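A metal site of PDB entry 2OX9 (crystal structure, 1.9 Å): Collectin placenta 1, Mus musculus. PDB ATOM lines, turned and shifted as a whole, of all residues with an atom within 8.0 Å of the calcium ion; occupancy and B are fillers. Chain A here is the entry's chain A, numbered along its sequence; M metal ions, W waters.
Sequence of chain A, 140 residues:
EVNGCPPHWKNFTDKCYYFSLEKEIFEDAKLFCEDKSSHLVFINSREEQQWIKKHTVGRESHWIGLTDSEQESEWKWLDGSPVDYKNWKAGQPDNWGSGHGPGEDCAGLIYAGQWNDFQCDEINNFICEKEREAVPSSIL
NZ of Lys 15 sits close to OE2 of Glu 129 (3.0 Å).
OE1 of Glu 48 sits close to OH of Tyr 17.
The side-chain carboxylate (OE2) of Glu 129 sits close to the side-chain hydroxyl (OH) of Tyr 17 (3.3 Å).
O of His 39 is in hydrogen-bond range of N of Glu 129 (2.8 Å).
The backbone NH (N) of Glu 48 lies within hydrogen-bond range of the side-chain hydroxyl (OG) of Ser 45, 3.3 Å away.
Of the 16 residues printed, 4 come within 4 Å of the calcium ion.
The nearest printed residue that does not touch the calcium ion is Tyr 17 (4.3 Å).
The calcium ion is bound by water W2, at 2.2 Å.
The calcium ion is bound by the backbone carbonyl oxygen (O) of Phe 42 (2.3 Å).
The calcium ion is bound by water W1 (2.4 Å).
The calcium ion is bound by the side-chain carboxylate (OE2) of Glu 129 (2.5 Å).
The calcium ion is bound by OE1 of Glu 48.
The calcium ion is bound by OD1 of Asn 44 (2.6 Å).
The side-chain carboxylate (OE1) of Glu 129 binds the calcium ion, 2.7 Å away.
The calcium ion has seven donor atoms within binding distance.
Slightly farther from the calcium ion lies OE2 of Glu 48 (2.9 Å).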
ATOM      1  N   PHE A  12     -19.184  14.245   5.053  1.00  0.00           N
ATOM      2  CA  PHE A  12     -18.961  13.002   5.778  1.00  0.00           C
ATOM      3  C   PHE A  12     -17.440  12.942   5.844  1.00  0.00           C
ATOM      4  O   PHE A  12     -16.780  12.862   4.820  1.00  0.00           O
ATOM      5  CB  PHE A  12     -19.486  11.795   5.016  1.00  0.00           C
ATOM      6  CG  PHE A  12     -19.225  10.494   5.725  1.00  0.00           C
ATOM      7  CD1 PHE A  12     -19.797  10.244   6.971  1.00  0.00           C
ATOM      8  CD2 PHE A  12     -18.405   9.527   5.162  1.00  0.00           C
ATOM      9  CE1 PHE A  12     -19.534   9.051   7.644  1.00  0.00           C
ATOM     10  CE2 PHE A  12     -18.136   8.335   5.827  1.00  0.00           C
ATOM     11  CZ  PHE A  12     -18.704   8.100   7.066  1.00  0.00           C
ATOM     12  N   THR A  13     -16.883  12.962   7.063  1.00  0.00           N
ATOM     13  CA  THR A  13     -15.439  12.990   7.250  1.00  0.00           C
ATOM     14  C   THR A  13     -14.913  14.180   6.448  1.00  0.00           C
ATOM     15  O   THR A  13     -15.475  15.274   6.555  1.00  0.00           O
ATOM     16  CB  THR A  13     -14.728  11.672   6.817  1.00  0.00           C
ATOM     17  OG1 THR A  13     -14.921  11.433   5.421  1.00  0.00           O
ATOM     18  CG2 THR A  13     -15.264  10.502   7.614  1.00  0.00           C
ATOM     19  N   LYS A  15     -14.933  14.612   3.111  1.00  0.00           N
ATOM     20  CA  LYS A  15     -15.452  14.597   1.750  1.00  0.00           C
ATOM     21  C   LYS A  15     -16.799  15.283   1.688  1.00  0.00           C
ATOM     22  O   LYS A  15     -17.446  15.503   2.719  1.00  0.00           O
ATOM     23  CB  LYS A  15     -15.596  13.156   1.267  1.00  0.00           C
ATOM     24  CG  LYS A  15     -14.287  12.385   1.182  1.00  0.00           C
ATOM     25  CD  LYS A  15     -13.239  13.183   0.419  1.00  0.00           C
ATOM     26  CE  LYS A  15     -12.434  12.263  -0.469  1.00  0.00           C
ATOM     27  NZ  LYS A  15     -13.303  11.572  -1.469  1.00  0.00           N
ATOM     28  N   TYR A  17     -20.521  15.285  -0.570  1.00  0.00           N
ATOM     29  CA  TYR A  17     -21.345  14.505  -1.474  1.00  0.00           C
ATOM     30  C   TYR A  17     -22.571  15.272  -1.934  1.00  0.00           C
ATOM     31  O   TYR A  17     -23.118  16.089  -1.194  1.00  0.00           O
ATOM     32  CB  TYR A  17     -21.823  13.228  -0.792  1.00  0.00           C
ATOM     33  CG  TYR A  17     -20.710  12.370  -0.217  1.00  0.00           C
ATOM     34  CD1 TYR A  17     -20.030  12.774   0.931  1.00  0.00           C
ATOM     35  CD2 TYR A  17     -20.349  11.172  -0.822  1.00  0.00           C
ATOM     36  CE1 TYR A  17     -19.010  11.990   1.472  1.00  0.00           C
ATOM     37  CE2 TYR A  17     -19.325  10.382  -0.293  1.00  0.00           C
ATOM     38  CZ  TYR A  17     -18.665  10.796   0.853  1.00  0.00           C
ATOM     39  OH  TYR A  17     -17.668  10.014   1.386  1.00  0.00           O
ATOM     40  N   HIS A  39     -16.545  13.211  -8.828  1.00  0.00           N
ATOM     41  CA  HIS A  39     -16.731  11.964  -9.568  1.00  0.00           C
ATOM     42  C   HIS A  39     -17.922  11.197  -9.003  1.00  0.00           C
ATOM     43  O   HIS A  39     -18.324  11.419  -7.865  1.00  0.00           O
ATOM     44  CB  HIS A  39     -15.476  11.087  -9.471  1.00  0.00           C
ATOM     45  CG  HIS A  39     -15.111  10.690  -8.073  1.00  0.00           C
ATOM     46  ND1 HIS A  39     -15.743   9.656  -7.414  1.00  0.00           N
ATOM     47  CD2 HIS A  39     -14.230  11.214  -7.199  1.00  0.00           C
ATOM     48  CE1 HIS A  39     -15.247   9.562  -6.188  1.00  0.00           C
ATOM     49  NE2 HIS A  39     -14.335  10.493  -6.034  1.00  0.00           N
ATOM     50  N   LEU A  40     -18.517  10.336  -9.815  1.00  0.00           N
ATOM     51  CA  LEU A  40     -19.629   9.518  -9.309  1.00  0.00           C
ATOM     52  C   LEU A  40     -19.030   8.818  -8.100  1.00  0.00           C
ATOM     53  O   LEU A  40     -17.918   8.312  -8.147  1.00  0.00           O
ATOM     54  CB  LEU A  40     -20.079   8.514 -10.368  1.00  0.00           C
ATOM     55  CG  LEU A  40     -20.998   9.088 -11.456  1.00  0.00           C
ATOM     56  CD1 LEU A  40     -21.155   8.069 -12.587  1.00  0.00           C
ATOM     57  CD2 LEU A  40     -22.361   9.413 -10.846  1.00  0.00           C
ATOM     58  N   VAL A  41     -19.784   8.809  -6.999  1.00  0.00           N
ATOM     59  CA  VAL A  41     -19.314   8.235  -5.739  1.00  0.00           C
ATOM     60  C   VAL A  41     -18.631   6.865  -5.722  1.00  0.00           C
ATOM     61  O   VAL A  41     -19.081   5.900  -6.360  1.00  0.00           O
ATOM     62  CB  VAL A  41     -20.498   8.217  -4.699  1.00  0.00           C
ATOM     63  CG1 VAL A  41     -21.426   7.021  -4.980  1.00  0.00           C
ATOM     64  CG2 VAL A  41     -19.947   8.154  -3.291  1.00  0.00           C
ATOM     65  N   PHE A  42     -17.518   6.797  -4.990  1.00  0.00           N
ATOM     66  CA  PHE A  42     -16.768   5.553  -4.794  1.00  0.00           C
ATOM     67  C   PHE A  42     -17.060   5.184  -3.345  1.00  0.00           C
ATOM     68  O   PHE A  42     -16.728   5.938  -2.424  1.00  0.00           O
ATOM     69  CB  PHE A  42     -15.256   5.767  -4.954  1.00  0.00           C
ATOM     70  CG  PHE A  42     -14.833   6.215  -6.321  1.00  0.00           C
ATOM     71  CD1 PHE A  42     -13.521   6.661  -6.535  1.00  0.00           C
ATOM     72  CD2 PHE A  42     -15.718   6.205  -7.391  1.00  0.00           C
ATOM     73  CE1 PHE A  42     -13.110   7.088  -7.792  1.00  0.00           C
ATOM     74  CE2 PHE A  42     -15.312   6.638  -8.653  1.00  0.00           C
ATOM     75  CZ  PHE A  42     -14.002   7.077  -8.855  1.00  0.00           C
ATOM     76  N   ILE A  43     -17.674   4.034  -3.117  1.00  0.00           N
ATOM     77  CA  ILE A  43     -18.007   3.612  -1.757  1.00  0.00           C
ATOM     78  C   ILE A  43     -16.944   2.625  -1.306  1.00  0.00           C
ATOM     79  O   ILE A  43     -16.947   1.467  -1.721  1.00  0.00           O
ATOM     80  CB  ILE A  43     -19.407   2.977  -1.727  1.00  0.00           C
ATOM     81  CG1 ILE A  43     -20.422   3.962  -2.340  1.00  0.00           C
ATOM     82  CG2 ILE A  43     -19.801   2.623  -0.289  1.00  0.00           C
ATOM     83  CD1 ILE A  43     -21.834   3.416  -2.430  1.00  0.00           C
ATOM     84  N   ASN A  44     -16.042   3.081  -0.438  1.00  0.00           N
ATOM     85  CA  ASN A  44     -14.921   2.287   0.044  1.00  0.00           C
ATOM     86  C   ASN A  44     -15.041   1.604   1.409  1.00  0.00           C
ATOM     87  O   ASN A  44     -14.108   0.915   1.814  1.00  0.00           O
ATOM     88  CB  ASN A  44     -13.653   3.149   0.065  1.00  0.00           C
ATOM     89  CG  ASN A  44     -13.565   4.104  -1.106  1.00  0.00           C
ATOM     90  OD1 ASN A  44     -14.177   5.178  -1.118  1.00  0.00           O
ATOM     91  ND2 ASN A  44     -12.801   3.713  -2.125  1.00  0.00           N
ATOM     92  N   SER A  45     -16.143   1.782   2.116  1.00  0.00           N
ATOM     93  CA  SER A  45     -16.273   1.161   3.427  1.00  0.00           C
ATOM     94  C   SER A  45     -17.727   1.038   3.877  1.00  0.00           C
ATOM     95  O   SER A  45     -18.610   1.683   3.319  1.00  0.00           O
ATOM     96  CB  SER A  45     -15.506   1.976   4.463  1.00  0.00           C
ATOM     97  OG  SER A  45     -16.082   3.257   4.643  1.00  0.00           O
ATOM     98  N   GLU A  48     -19.086   4.468   5.141  1.00  0.00           N
ATOM     99  CA  GLU A  48     -19.468   5.412   4.094  1.00  0.00           C
ATOM    100  C   GLU A  48     -20.770   4.917   3.450  1.00  0.00           C
ATOM    101  O   GLU A  48     -21.639   5.707   3.080  1.00  0.00           O
ATOM    102  CB  GLU A  48     -18.357   5.515   3.026  1.00  0.00           C
ATOM    103  CG  GLU A  48     -18.633   6.573   1.958  1.00  0.00           C
ATOM    104  CD  GLU A  48     -17.525   6.698   0.919  1.00  0.00           C
ATOM    105  OE1 GLU A  48     -17.470   7.738   0.244  1.00  0.00           O
ATOM    106  OE2 GLU A  48     -16.719   5.753   0.775  1.00  0.00           O
ATOM    107  N   ILE A  52     -24.329   6.882   3.357  1.00  0.00           N
ATOM    108  CA  ILE A  52     -24.947   7.136   2.056  1.00  0.00           C
ATOM    109  C   ILE A  52     -26.366   6.583   2.026  1.00  0.00           C
ATOM    110  O   ILE A  52     -27.280   7.215   1.492  1.00  0.00           O
ATOM    111  CB  ILE A  52     -24.125   6.494   0.912  1.00  0.00           C
ATOM    112  CG1 ILE A  52     -22.884   7.351   0.645  1.00  0.00           C
ATOM    113  CG2 ILE A  52     -24.961   6.395  -0.361  1.00  0.00           C
ATOM    114  CD1 ILE A  52     -21.954   6.761  -0.416  1.00  0.00           C
ATOM    115  N   TRP A  77     -13.891   0.953  -9.951  1.00  0.00           N
ATOM    116  CA  TRP A  77     -14.380   2.317  -9.786  1.00  0.00           C
ATOM    117  C   TRP A  77     -13.841   3.117 -10.973  1.00  0.00           C
ATOM    118  O   TRP A  77     -12.875   2.696 -11.627  1.00  0.00           O
ATOM    119  CB  TRP A  77     -13.889   2.896  -8.455  1.00  0.00           C
ATOM    120  CG  TRP A  77     -14.436   2.159  -7.265  1.00  0.00           C
ATOM    121  CD1 TRP A  77     -13.766   1.268  -6.464  1.00  0.00           C
ATOM    122  CD2 TRP A  77     -15.781   2.196  -6.769  1.00  0.00           C
ATOM    123  NE1 TRP A  77     -14.605   0.762  -5.510  1.00  0.00           N
ATOM    124  CE2 TRP A  77     -15.842   1.309  -5.672  1.00  0.00           C
ATOM    125  CE3 TRP A  77     -16.930   2.908  -7.152  1.00  0.00           C
ATOM    126  CZ2 TRP A  77     -17.030   1.103  -4.943  1.00  0.00           C
ATOM    127  CZ3 TRP A  77     -18.105   2.697  -6.425  1.00  0.00           C
ATOM    128  CH2 TRP A  77     -18.146   1.806  -5.337  1.00  0.00           C
ATOM    129  N   GLU A 129     -19.001  12.820  -5.520  1.00  0.00           N
ATOM    130  CA  GLU A 129     -18.128  12.888  -4.369  1.00  0.00           C
ATOM    131  C   GLU A 129     -16.872  13.703  -4.684  1.00  0.00           C
ATOM    132  O   GLU A 129     -16.321  13.627  -5.783  1.00  0.00           O
ATOM    133  CB  GLU A 129     -17.735  11.462  -3.929  1.00  0.00           C
ATOM    134  CG  GLU A 129     -16.665  11.431  -2.845  1.00  0.00           C
ATOM    135  CD  GLU A 129     -16.275  10.027  -2.418  1.00  0.00           C
ATOM    136  OE1 GLU A 129     -16.467   9.060  -3.186  1.00  0.00           O
ATOM    137  OE2 GLU A 129     -15.749   9.893  -1.295  1.00  0.00           O
ATOM    138  N   LYS A 130     -16.426  14.473  -3.709  1.00  0.00           N
ATOM    139  CA  LYS A 130     -15.219  15.260  -3.896  1.00  0.00           C
ATOM    140  C   LYS A 130     -14.624  15.680  -2.562  1.00  0.00           C
ATOM    141  O   LYS A 130     -15.225  15.484  -1.514  1.00  0.00           O
ATOM    142  CB  LYS A 130     -15.477  16.492  -4.766  1.00  0.00           C
ATOM    143  CG  LYS A 130     -16.336  17.583  -4.150  1.00  0.00           C
ATOM    144  CD  LYS A 130     -16.443  18.742  -5.139  1.00  0.00           C
ATOM    145  CE  LYS A 130     -17.234  19.924  -4.582  1.00  0.00           C
ATOM    146  NZ  LYS A 130     -17.281  21.059  -5.574  1.00  0.00           N
HETATM  147 CA    CA M   1     -15.475   7.439  -1.234  1.00  0.00          CA
HETATM  148  O   HOH W   1     -13.609   7.627  -2.683  1.00  0.00           O
HETATM  149  O   HOH W   2     -13.981   8.075   0.318  1.00  0.00           O
